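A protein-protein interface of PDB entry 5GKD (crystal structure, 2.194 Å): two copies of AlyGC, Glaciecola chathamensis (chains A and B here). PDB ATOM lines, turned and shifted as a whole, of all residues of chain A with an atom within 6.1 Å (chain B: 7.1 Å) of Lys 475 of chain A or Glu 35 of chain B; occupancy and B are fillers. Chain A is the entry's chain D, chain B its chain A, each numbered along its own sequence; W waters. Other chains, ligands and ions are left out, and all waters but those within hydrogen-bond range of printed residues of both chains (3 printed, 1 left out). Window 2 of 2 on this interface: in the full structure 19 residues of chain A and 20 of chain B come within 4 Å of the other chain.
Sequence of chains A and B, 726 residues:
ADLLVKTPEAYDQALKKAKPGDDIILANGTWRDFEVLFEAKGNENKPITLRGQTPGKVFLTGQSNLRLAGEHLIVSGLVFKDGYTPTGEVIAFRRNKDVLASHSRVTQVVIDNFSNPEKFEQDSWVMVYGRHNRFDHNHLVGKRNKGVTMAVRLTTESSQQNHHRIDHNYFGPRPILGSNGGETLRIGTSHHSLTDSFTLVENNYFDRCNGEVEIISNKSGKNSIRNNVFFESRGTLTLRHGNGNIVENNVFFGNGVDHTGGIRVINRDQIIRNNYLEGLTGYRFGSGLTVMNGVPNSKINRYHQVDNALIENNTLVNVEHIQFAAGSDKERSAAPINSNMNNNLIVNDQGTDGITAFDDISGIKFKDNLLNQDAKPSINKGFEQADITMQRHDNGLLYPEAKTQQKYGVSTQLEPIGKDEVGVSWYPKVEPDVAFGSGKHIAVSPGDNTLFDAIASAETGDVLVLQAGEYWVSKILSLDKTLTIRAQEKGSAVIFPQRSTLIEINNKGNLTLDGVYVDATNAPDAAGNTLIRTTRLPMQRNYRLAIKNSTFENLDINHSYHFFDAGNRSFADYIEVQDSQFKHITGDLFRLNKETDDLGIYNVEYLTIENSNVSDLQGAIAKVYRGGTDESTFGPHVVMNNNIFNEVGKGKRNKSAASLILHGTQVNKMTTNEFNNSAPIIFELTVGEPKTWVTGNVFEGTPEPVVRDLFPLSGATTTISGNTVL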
ATOM      1  N   ASN A 449      24.944  19.045   5.951  1.00  0.00           N
ATOM      2  CA  ASN A 449      23.513  19.331   5.805  1.00  0.00           C
ATOM      3  C   ASN A 449      22.631  18.084   5.934  1.00  0.00           C
ATOM      4  O   ASN A 449      21.504  18.066   5.436  1.00  0.00           O
ATOM      5  CB  ASN A 449      23.221  20.068   4.498  1.00  0.00           C
ATOM      6  CG  ASN A 449      23.760  21.483   4.513  1.00  0.00           C
ATOM      7  OD1 ASN A 449      23.817  22.127   5.565  1.00  0.00           O
ATOM      8  ND2 ASN A 449      24.195  21.960   3.357  1.00  0.00           N
ATOM      9  N   PHE A 452      20.017  19.560   8.230  1.00  0.00           N
ATOM     10  CA  PHE A 452      19.106  20.339   7.400  1.00  0.00           C
ATOM     11  C   PHE A 452      18.106  19.446   6.673  1.00  0.00           C
ATOM     12  O   PHE A 452      16.909  19.730   6.651  1.00  0.00           O
ATOM     13  CB  PHE A 452      19.908  21.167   6.390  1.00  0.00           C
ATOM     14  CG  PHE A 452      19.052  21.973   5.443  1.00  0.00           C
ATOM     15  CD1 PHE A 452      18.650  23.250   5.775  1.00  0.00           C
ATOM     16  CD2 PHE A 452      18.660  21.454   4.217  1.00  0.00           C
ATOM     17  CE1 PHE A 452      17.868  23.994   4.910  1.00  0.00           C
ATOM     18  CE2 PHE A 452      17.877  22.195   3.346  1.00  0.00           C
ATOM     19  CZ  PHE A 452      17.483  23.467   3.695  1.00  0.00           C
ATOM     20  N   ASP A 453      18.591  18.374   6.049  1.00  0.00           N
ATOM     21  CA  ASP A 453      17.719  17.484   5.291  1.00  0.00           C
ATOM     22  C   ASP A 453      16.740  16.757   6.197  1.00  0.00           C
ATOM     23  O   ASP A 453      15.551  16.661   5.884  1.00  0.00           O
ATOM     24  CB  ASP A 453      18.545  16.467   4.501  1.00  0.00           C
ATOM     25  CG  ASP A 453      19.351  17.111   3.385  1.00  0.00           C
ATOM     26  OD1 ASP A 453      18.918  18.167   2.858  1.00  0.00           O
ATOM     27  OD2 ASP A 453      20.416  16.550   3.042  1.00  0.00           O
ATOM     28  N   VAL A 473      26.735  22.605   9.602  1.00  0.00           N
ATOM     29  CA  VAL A 473      25.458  23.235   9.268  1.00  0.00           C
ATOM     30  C   VAL A 473      25.758  24.529   8.520  1.00  0.00           C
ATOM     31  O   VAL A 473      26.018  25.566   9.142  1.00  0.00           O
ATOM     32  CB  VAL A 473      24.606  23.515  10.504  1.00  0.00           C
ATOM     33  CG1 VAL A 473      23.322  24.162  10.098  1.00  0.00           C
ATOM     34  CG2 VAL A 473      24.324  22.239  11.258  1.00  0.00           C
ATOM     35  N   SER A 474      25.727  24.472   7.187  1.00  0.00           N
ATOM     36  CA  SER A 474      26.003  25.626   6.335  1.00  0.00           C
ATOM     37  C   SER A 474      24.738  26.330   5.866  1.00  0.00           C
ATOM     38  O   SER A 474      24.828  27.303   5.122  1.00  0.00           O
ATOM     39  CB  SER A 474      26.839  25.216   5.120  1.00  0.00           C
ATOM     40  OG  SER A 474      26.178  24.230   4.348  1.00  0.00           O
ATOM     41  N   LYS A 475      23.572  25.859   6.284  1.00  0.00           N
ATOM     42  CA  LYS A 475      22.304  26.523   6.009  1.00  0.00           C
ATOM     43  C   LYS A 475      21.559  26.675   7.323  1.00  0.00           C
ATOM     44  O   LYS A 475      21.610  25.781   8.168  1.00  0.00           O
ATOM     45  CB  LYS A 475      21.426  25.729   5.024  1.00  0.00           C
ATOM     46  CG  LYS A 475      22.061  25.401   3.702  1.00  0.00           C
ATOM     47  CD  LYS A 475      20.986  24.853   2.787  1.00  0.00           C
ATOM     48  CE  LYS A 475      21.499  23.849   1.807  1.00  0.00           C
ATOM     49  NZ  LYS A 475      20.372  23.300   0.980  1.00  0.00           N
ATOM     50  N   ILE A 476      20.842  27.789   7.476  1.00  0.00           N
ATOM     51  CA  ILE A 476      20.001  27.988   8.648  1.00  0.00           C
ATOM     52  C   ILE A 476      18.958  26.875   8.751  1.00  0.00           C
ATOM     53  O   ILE A 476      18.285  26.536   7.770  1.00  0.00           O
ATOM     54  CB  ILE A 476      19.345  29.376   8.589  1.00  0.00           C
ATOM     55  CG1 ILE A 476      20.388  30.462   8.851  1.00  0.00           C
ATOM     56  CG2 ILE A 476      18.212  29.498   9.600  1.00  0.00           C
ATOM     57  CD1 ILE A 476      19.805  31.902   8.696  1.00  0.00           C
ATOM     58  N   LEU A 477      18.847  26.284   9.944  1.00  0.00           N
ATOM     59  CA  LEU A 477      17.839  25.274  10.280  1.00  0.00           C
ATOM     60  C   LEU A 477      16.540  25.987  10.651  1.00  0.00           C
ATOM     61  O   LEU A 477      16.426  26.559  11.734  1.00  0.00           O
ATOM     62  CB  LEU A 477      18.319  24.414  11.443  1.00  0.00           C
ATOM     63  CG  LEU A 477      19.267  23.212  11.290  1.00  0.00           C
ATOM     64  CD1 LEU A 477      19.962  23.188   9.969  1.00  0.00           C
ATOM     65  CD2 LEU A 477      20.258  23.136  12.423  1.00  0.00           C
ATOM     66  N   ARG A 499      26.687  29.385  10.010  1.00  0.00           N
ATOM     67  CA  ARG A 499      25.943  30.606   9.746  1.00  0.00           C
ATOM     68  C   ARG A 499      25.771  31.407  11.030  1.00  0.00           C
ATOM     69  O   ARG A 499      25.969  30.906  12.135  1.00  0.00           O
ATOM     70  CB  ARG A 499      24.560  30.293   9.153  1.00  0.00           C
ATOM     71  CG  ARG A 499      24.542  29.431   7.884  1.00  0.00           C
ATOM     72  CD  ARG A 499      24.629  30.288   6.619  1.00  0.00           C
ATOM     73  NE  ARG A 499      25.856  31.070   6.616  1.00  0.00           N
ATOM     74  CZ  ARG A 499      26.992  30.650   6.070  1.00  0.00           C
ATOM     75  NH1 ARG A 499      27.069  29.454   5.488  1.00  0.00           N
ATOM     76  NH2 ARG A 499      28.077  31.414   6.141  1.00  0.00           N
ATOM     77  N   THR A 501      23.078  32.255  12.316  1.00  0.00           N
ATOM     78  CA  THR A 501      22.023  31.588  13.057  1.00  0.00           C
ATOM     79  C   THR A 501      22.140  30.090  12.824  1.00  0.00           C
ATOM     80  O   THR A 501      22.386  29.650  11.697  1.00  0.00           O
ATOM     81  CB  THR A 501      20.630  32.080  12.628  1.00  0.00           C
ATOM     82  OG1 THR A 501      20.419  33.387  13.143  1.00  0.00           O
ATOM     83  CG2 THR A 501      19.538  31.184  13.182  1.00  0.00           C
ATOM     84  N   LEU A 502      22.010  29.319  13.902  1.00  0.00           N
ATOM     85  CA  LEU A 502      21.894  27.867  13.807  1.00  0.00           C
ATOM     86  C   LEU A 502      20.439  27.450  13.608  1.00  0.00           C
ATOM     87  O   LEU A 502      20.103  26.804  12.612  1.00  0.00           O
ATOM     88  CB  LEU A 502      22.478  27.186  15.051  1.00  0.00           C
ATOM     89  CG  LEU A 502      22.388  25.653  15.058  1.00  0.00           C
ATOM     90  CD1 LEU A 502      23.143  25.076  13.870  1.00  0.00           C
ATOM     91  CD2 LEU A 502      22.919  25.050  16.344  1.00  0.00           C
ATOM     92  N   PRO B   8      18.192  19.114 -13.156  1.00  0.00           N
ATOM     93  CA  PRO B   8      19.343  18.895 -12.268  1.00  0.00           C
ATOM     94  C   PRO B   8      19.863  17.466 -12.301  1.00  0.00           C
ATOM     95  O   PRO B   8      21.074  17.255 -12.221  1.00  0.00           O
ATOM     96  CB  PRO B   8      18.798  19.285 -10.888  1.00  0.00           C
ATOM     97  CG  PRO B   8      17.773  20.286 -11.184  1.00  0.00           C
ATOM     98  CD  PRO B   8      17.113  19.844 -12.478  1.00  0.00           C
ATOM     99  N   TYR B  11      21.846  17.101 -15.321  1.00  0.00           N
ATOM    100  CA  TYR B  11      23.110  17.755 -15.033  1.00  0.00           C
ATOM    101  C   TYR B  11      24.046  16.828 -14.268  1.00  0.00           C
ATOM    102  O   TYR B  11      25.219  16.699 -14.617  1.00  0.00           O
ATOM    103  CB  TYR B  11      22.882  19.046 -14.254  1.00  0.00           C
ATOM    104  CG  TYR B  11      24.166  19.539 -13.638  1.00  0.00           C
ATOM    105  CD1 TYR B  11      25.052  20.317 -14.364  1.00  0.00           C
ATOM    106  CD2 TYR B  11      24.501  19.203 -12.342  1.00  0.00           C
ATOM    107  CE1 TYR B  11      26.223  20.763 -13.810  1.00  0.00           C
ATOM    108  CE2 TYR B  11      25.671  19.626 -11.787  1.00  0.00           C
ATOM    109  CZ  TYR B  11      26.526  20.413 -12.519  1.00  0.00           C
ATOM    110  OH  TYR B  11      27.687  20.824 -11.928  1.00  0.00           O
ATOM    111  N   ASP B  12      23.550  16.190 -13.206  1.00  0.00           N
ATOM    112  CA  ASP B  12      24.383  15.256 -12.454  1.00  0.00           C
ATOM    113  C   ASP B  12      24.995  14.208 -13.367  1.00  0.00           C
ATOM    114  O   ASP B  12      26.180  13.875 -13.244  1.00  0.00           O
ATOM    115  CB  ASP B  12      23.568  14.550 -11.356  1.00  0.00           C
ATOM    116  CG  ASP B  12      23.144  15.483 -10.227  1.00  0.00           C
ATOM    117  OD1 ASP B  12      23.812  16.516  -9.995  1.00  0.00           O
ATOM    118  OD2 ASP B  12      22.139  15.167  -9.566  1.00  0.00           O
ATOM    119  N   ARG B  32      14.890  26.777 -10.983  1.00  0.00           N
ATOM    120  CA  ARG B  32      14.567  27.276  -9.657  1.00  0.00           C
ATOM    121  C   ARG B  32      15.169  26.368  -8.591  1.00  0.00           C
ATOM    122  O   ARG B  32      15.195  25.147  -8.744  1.00  0.00           O
ATOM    123  CB  ARG B  32      13.050  27.400  -9.470  1.00  0.00           C
ATOM    124  CG  ARG B  32      12.648  28.048  -8.143  1.00  0.00           C
ATOM    125  CD  ARG B  32      11.531  29.084  -8.256  1.00  0.00           C
ATOM    126  NE  ARG B  32      11.311  29.726  -6.957  1.00  0.00           N
ATOM    127  CZ  ARG B  32      11.454  31.030  -6.681  1.00  0.00           C
ATOM    128  NH1 ARG B  32      11.801  31.918  -7.620  1.00  0.00           N
ATOM    129  NH2 ARG B  32      11.240  31.451  -5.439  1.00  0.00           N
ATOM    130  N   ASP B  33      15.676  26.975  -7.521  1.00  0.00           N
ATOM    131  CA  ASP B  33      16.228  26.230  -6.390  1.00  0.00           C
ATOM    132  C   ASP B  33      17.307  25.244  -6.837  1.00  0.00           C
ATOM    133  O   ASP B  33      17.336  24.096  -6.405  1.00  0.00           O
ATOM    134  CB  ASP B  33      15.122  25.489  -5.629  1.00  0.00           C
ATOM    135  CG  ASP B  33      14.019  26.414  -5.125  1.00  0.00           C
ATOM    136  OD1 ASP B  33      14.263  27.613  -4.890  1.00  0.00           O
ATOM    137  OD2 ASP B  33      12.893  25.920  -4.951  1.00  0.00           O
ATOM    138  N   PHE B  34      18.198  25.694  -7.716  1.00  0.00           N
ATOM    139  CA  PHE B  34      19.251  24.858  -8.282  1.00  0.00           C
ATOM    140  C   PHE B  34      20.579  25.212  -7.614  1.00  0.00           C
ATOM    141  O   PHE B  34      21.215  26.202  -7.976  1.00  0.00           O
ATOM    142  CB  PHE B  34      19.327  25.052  -9.793  1.00  0.00           C
ATOM    143  CG  PHE B  34      20.187  24.035 -10.503  1.00  0.00           C
ATOM    144  CD1 PHE B  34      20.601  22.877  -9.859  1.00  0.00           C
ATOM    145  CD2 PHE B  34      20.581  24.238 -11.812  1.00  0.00           C
ATOM    146  CE1 PHE B  34      21.375  21.947 -10.515  1.00  0.00           C
ATOM    147  CE2 PHE B  34      21.373  23.302 -12.461  1.00  0.00           C
ATOM    148  CZ  PHE B  34      21.764  22.162 -11.811  1.00  0.00           C
ATOM    149  N   GLU B  35      21.007  24.379  -6.662  1.00  0.00           N
ATOM    150  CA  GLU B  35      22.319  24.502  -6.023  1.00  0.00           C
ATOM    151  C   GLU B  35      23.334  23.739  -6.866  1.00  0.00           C
ATOM    152  O   GLU B  35      23.445  22.519  -6.767  1.00  0.00           O
ATOM    153  CB  GLU B  35      22.280  23.974  -4.593  1.00  0.00           C
ATOM    154  CG  GLU B  35      21.432  24.800  -3.660  1.00  0.00           C
ATOM    155  CD  GLU B  35      21.408  24.266  -2.234  1.00  0.00           C
ATOM    156  OE1 GLU B  35      22.426  24.392  -1.518  1.00  0.00           O
ATOM    157  OE2 GLU B  35      20.360  23.741  -1.825  1.00  0.00           O
ATOM    158  N   VAL B  36      24.084  24.461  -7.695  1.00  0.00           N
ATOM    159  CA  VAL B  36      24.981  23.862  -8.673  1.00  0.00           C
ATOM    160  C   VAL B  36      26.313  23.567  -8.001  1.00  0.00           C
ATOM    161  O   VAL B  36      26.949  24.468  -7.455  1.00  0.00           O
ATOM    162  CB  VAL B  36      25.183  24.786  -9.882  1.00  0.00           C
ATOM    163  CG1 VAL B  36      26.161  24.165 -10.866  1.00  0.00           C
ATOM    164  CG2 VAL B  36      23.843  25.110 -10.544  1.00  0.00           C
ATOM    165  N   LEU B  37      26.742  22.311  -8.042  1.00  0.00           N
ATOM    166  CA  LEU B  37      28.089  21.928  -7.637  1.00  0.00           C
ATOM    167  C   LEU B  37      28.800  21.464  -8.897  1.00  0.00           C
ATOM    168  O   LEU B  37      28.515  20.378  -9.414  1.00  0.00           O
ATOM    169  CB  LEU B  37      28.086  20.844  -6.560  1.00  0.00           C
ATOM    170  CG  LEU B  37      29.454  20.257  -6.164  1.00  0.00           C
ATOM    171  CD1 LEU B  37      30.417  21.360  -5.772  1.00  0.00           C
ATOM    172  CD2 LEU B  37      29.333  19.227  -5.038  1.00  0.00           C
ATOM    173  N   PHE B  38      29.695  22.311  -9.405  1.00  0.00           N
ATOM    174  CA  PHE B  38      30.456  22.063 -10.624  1.00  0.00           C
ATOM    175  C   PHE B  38      31.825  21.570 -10.182  1.00  0.00           C
ATOM    176  O   PHE B  38      32.748  22.353  -9.968  1.00  0.00           O
ATOM    177  CB  PHE B  38      30.561  23.327 -11.464  1.00  0.00           C
ATOM    178  CG  PHE B  38      31.169  23.107 -12.821  1.00  0.00           C
ATOM    179  CD1 PHE B  38      30.896  21.965 -13.543  1.00  0.00           C
ATOM    180  CD2 PHE B  38      31.989  24.053 -13.380  1.00  0.00           C
ATOM    181  CE1 PHE B  38      31.453  21.784 -14.793  1.00  0.00           C
ATOM    182  CE2 PHE B  38      32.537  23.875 -14.635  1.00  0.00           C
ATOM    183  CZ  PHE B  38      32.279  22.750 -15.334  1.00  0.00           C
ATOM    184  N   LEU B  60      18.924  31.240 -13.065  1.00  0.00           N
ATOM    185  CA  LEU B  60      18.972  30.449 -11.848  1.00  0.00           C
ATOM    186  C   LEU B  60      18.303  31.277 -10.764  1.00  0.00           C
ATOM    187  O   LEU B  60      18.815  32.333 -10.381  1.00  0.00           O
ATOM    188  CB  LEU B  60      20.400  30.072 -11.473  1.00  0.00           C
ATOM    189  CG  LEU B  60      20.864  28.765 -12.113  1.00  0.00           C
ATOM    190  CD1 LEU B  60      21.028  28.947 -13.591  1.00  0.00           C
ATOM    191  CD2 LEU B  60      22.137  28.239 -11.499  1.00  0.00           C
ATOM    192  N   GLN B  63      16.347  29.630  -4.434  1.00  0.00           N
ATOM    193  CA  GLN B  63      17.514  29.335  -3.600  1.00  0.00           C
ATOM    194  C   GLN B  63      18.521  28.524  -4.410  1.00  0.00           C
ATOM    195  O   GLN B  63      18.779  27.354  -4.154  1.00  0.00           O
ATOM    196  CB  GLN B  63      17.100  28.635  -2.312  1.00  0.00           C
ATOM    197  CG  GLN B  63      16.621  29.612  -1.250  1.00  0.00           C
ATOM    198  CD  GLN B  63      15.447  30.444  -1.748  1.00  0.00           C
ATOM    199  OE1 GLN B  63      14.318  29.955  -1.819  1.00  0.00           O
ATOM    200  NE2 GLN B  63      15.715  31.678  -2.148  1.00  0.00           N
ATOM    201  N   SER B  64      19.083  29.195  -5.417  1.00  0.00           N
ATOM    202  CA  SER B  64      20.115  28.673  -6.297  1.00  0.00           C
ATOM    203  C   SER B  64      21.462  29.246  -5.892  1.00  0.00           C
ATOM    204  O   SER B  64      21.542  30.312  -5.278  1.00  0.00           O
ATOM    205  CB  SER B  64      19.836  29.037  -7.756  1.00  0.00           C
ATOM    206  OG  SER B  64      18.702  28.391  -8.263  1.00  0.00           O
ATOM    207  N   ASN B  65      22.521  28.530  -6.249  1.00  0.00           N
ATOM    208  CA  ASN B  65      23.877  29.017  -6.031  1.00  0.00           C
ATOM    209  C   ASN B  65      24.813  28.182  -6.898  1.00  0.00           C
ATOM    210  O   ASN B  65      24.373  27.316  -7.656  1.00  0.00           O
ATOM    211  CB  ASN B  65      24.252  28.993  -4.542  1.00  0.00           C
ATOM    212  CG  ASN B  65      24.289  27.582  -3.948  1.00  0.00           C
ATOM    213  OD1 ASN B  65      24.390  26.592  -4.660  1.00  0.00           O
ATOM    214  ND2 ASN B  65      24.213  27.502  -2.627  1.00  0.00           N
ATOM    215  N   LEU B  66      26.110  28.463  -6.799  1.00  0.00           N
ATOM    216  CA  LEU B  66      27.105  27.812  -7.645  1.00  0.00           C
ATOM    217  C   LEU B  66      28.391  27.594  -6.866  1.00  0.00           C
ATOM    218  O   LEU B  66      28.889  28.514  -6.208  1.00  0.00           O
ATOM    219  CB  LEU B  66      27.388  28.637  -8.904  1.00  0.00           C
ATOM    220  CG  LEU B  66      28.606  28.265  -9.763  1.00  0.00           C
ATOM    221  CD1 LEU B  66      28.479  26.865 -10.325  1.00  0.00           C
ATOM    222  CD2 LEU B  66      28.800  29.271 -10.885  1.00  0.00           C
ATOM    223  N   ARG B  67      28.913  26.374  -6.928  1.00  0.00           N
ATOM    224  CA  ARG B  67      30.205  26.046  -6.343  1.00  0.00           C
ATOM    225  C   ARG B  67      31.069  25.411  -7.416  1.00  0.00           C
ATOM    226  O   ARG B  67      30.599  24.544  -8.156  1.00  0.00           O
ATOM    227  CB  ARG B  67      30.061  25.113  -5.138  1.00  0.00           C
ATOM    228  CG  ARG B  67      29.485  25.801  -3.895  1.00  0.00           C
ATOM    229  CD  ARG B  67      29.265  24.836  -2.750  1.00  0.00           C
ATOM    230  NE  ARG B  67      28.250  23.840  -3.072  1.00  0.00           N
ATOM    231  CZ  ARG B  67      28.121  22.659  -2.473  1.00  0.00           C
ATOM    232  NH1 ARG B  67      28.967  22.291  -1.510  1.00  0.00           N
ATOM    233  NH2 ARG B  67      27.147  21.839  -2.849  1.00  0.00           N
ATOM    234  N   THR B  85      20.914  33.098  -2.318  1.00  0.00           N
ATOM    235  CA  THR B  85      21.584  31.853  -1.990  1.00  0.00           C
ATOM    236  C   THR B  85      21.147  31.363  -0.610  1.00  0.00           C
ATOM    237  O   THR B  85      21.031  32.157   0.327  1.00  0.00           O
ATOM    238  CB  THR B  85      23.100  32.004  -2.015  1.00  0.00           C
ATOM    239  OG1 THR B  85      23.679  30.731  -1.698  1.00  0.00           O
ATOM    240  CG2 THR B  85      23.590  33.050  -0.997  1.00  0.00           C
ATOM    241  N   PRO B  86      20.868  30.066  -0.466  1.00  0.00           N
ATOM    242  CA  PRO B  86      20.594  29.510   0.863  1.00  0.00           C
ATOM    243  C   PRO B  86      21.851  29.269   1.690  1.00  0.00           C
ATOM    244  O   PRO B  86      21.734  28.957   2.884  1.00  0.00           O
ATOM    245  CB  PRO B  86      19.891  28.189   0.535  1.00  0.00           C
ATOM    246  CG  PRO B  86      20.520  27.777  -0.733  1.00  0.00           C
ATOM    247  CD  PRO B  86      20.791  29.037  -1.517  1.00  0.00           C
ATOM    248  N   THR B  87      23.044  29.392   1.105  1.00  0.00           N
ATOM    249  CA  THR B  87      24.274  29.197   1.865  1.00  0.00           C
ATOM    250  C   THR B  87      24.910  30.554   2.165  1.00  0.00           C
ATOM    251  O   THR B  87      24.228  31.593   2.191  1.00  0.00           O
ATOM    252  CB  THR B  87      25.227  28.248   1.117  1.00  0.00           C
ATOM    253  OG1 THR B  87      25.596  28.807  -0.141  1.00  0.00           O
ATOM    254  CG2 THR B  87      24.574  26.887   0.874  1.00  0.00           C
ATOM    255  N   GLY B  88      26.217  30.548   2.402  1.00  0.00           N
ATOM    256  CA  GLY B  88      26.911  31.785   2.673  1.00  0.00           C
ATOM    257  C   GLY B  88      27.246  32.593   1.444  1.00  0.00           C
ATOM    258  O   GLY B  88      27.573  33.774   1.576  1.00  0.00           O
HETATM  259  O   HOH W   1      18.326  24.888   0.499  1.00  0.00           O
HETATM  260  O   HOH W   2      28.402  28.764   2.514  1.00  0.00           O
HETATM  261  O   HOH W   3      20.614  29.625   5.345  1.00  0.00           O
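The side-chain carboxylate of Glu 35 of chain B is in salt-bridge range of the side-chain amino group of Lys 475 of chain A, 2.8 Å away. The backbone NH of Gly 88 of chain B lies close to the guanidinium group of Arg 499 of chain A, at 3.4 Å.
The side-chain amide nitrogen (ND2) of Asn 65 of chain B sits at hydrogen-bond distance from the side-chain hydroxyl (OG1) of Thr 87 of chain B, 3.1 Å away. The side-chain hydroxyl of Thr 87 of chain B sits at hydrogen-bond distance from the side-chain hydroxyl of Thr 85 of chain B (3.1 Å). The side-chain amide nitrogen (ND2) of Asn 449 of chain A sits at hydrogen-bond distance from the side-chain hydroxyl (OG) of Ser 474 of chain A, 3.2 Å away. NH1 of Arg 499 of chain A lies within hydrogen-bond range of O of Ser 474 of chain A (3.1 Å).
Among the printed residues, merely in contact across the chains: Lys 475 of chain A with Pro 86 of chain B (3.7 Å) and Ser 474 of chain A with Thr 87 of chain B (3.8 Å).
Of the printed residues of chain B, Ser 474 of chain A touches Thr 87. Printed residues of chain A within 4 Å of Glu 35 of chain B: Lys 475. Of the printed residues of chain A, Thr 87 of chain B touches Ser 474. Of the printed residues of chain A, Gly 88 of chain B touches Arg 499. The nearest residue of chain A that does not touch Glu 35 of chain B is Asn 449 of chain A (5.7 Å). The nearest printed residue of chain B that does not touch Ser 474 of chain A is Pro 86 of chain B (4.2 Å).
Among the printed residues, Asp or Glu carboxylates within 4 Å of a Lys or Arg side-chain nitrogen of the other chain: Lys 475 of chain A with Glu 35 of chain B.
No position is printed for both chains. Of the 4 pairs that touch across the chains among the printed residues, none has its exchanged pair printed and touching as well.
Water W1 bridges the side-chain amino group (NZ) of Lys 475 of chain A and the side-chain carboxylate (OE2) of Glu 35 of chain B. Water W3 bridges O of Pro 86 of chain B and N of Ile 476 of chain A. Water W2 lies within hydrogen-bond range of the backbone NH of Gly 88 of chain B (2.8 Å) and the guanidinium group of Arg 499 of chain A (3.3 Å).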
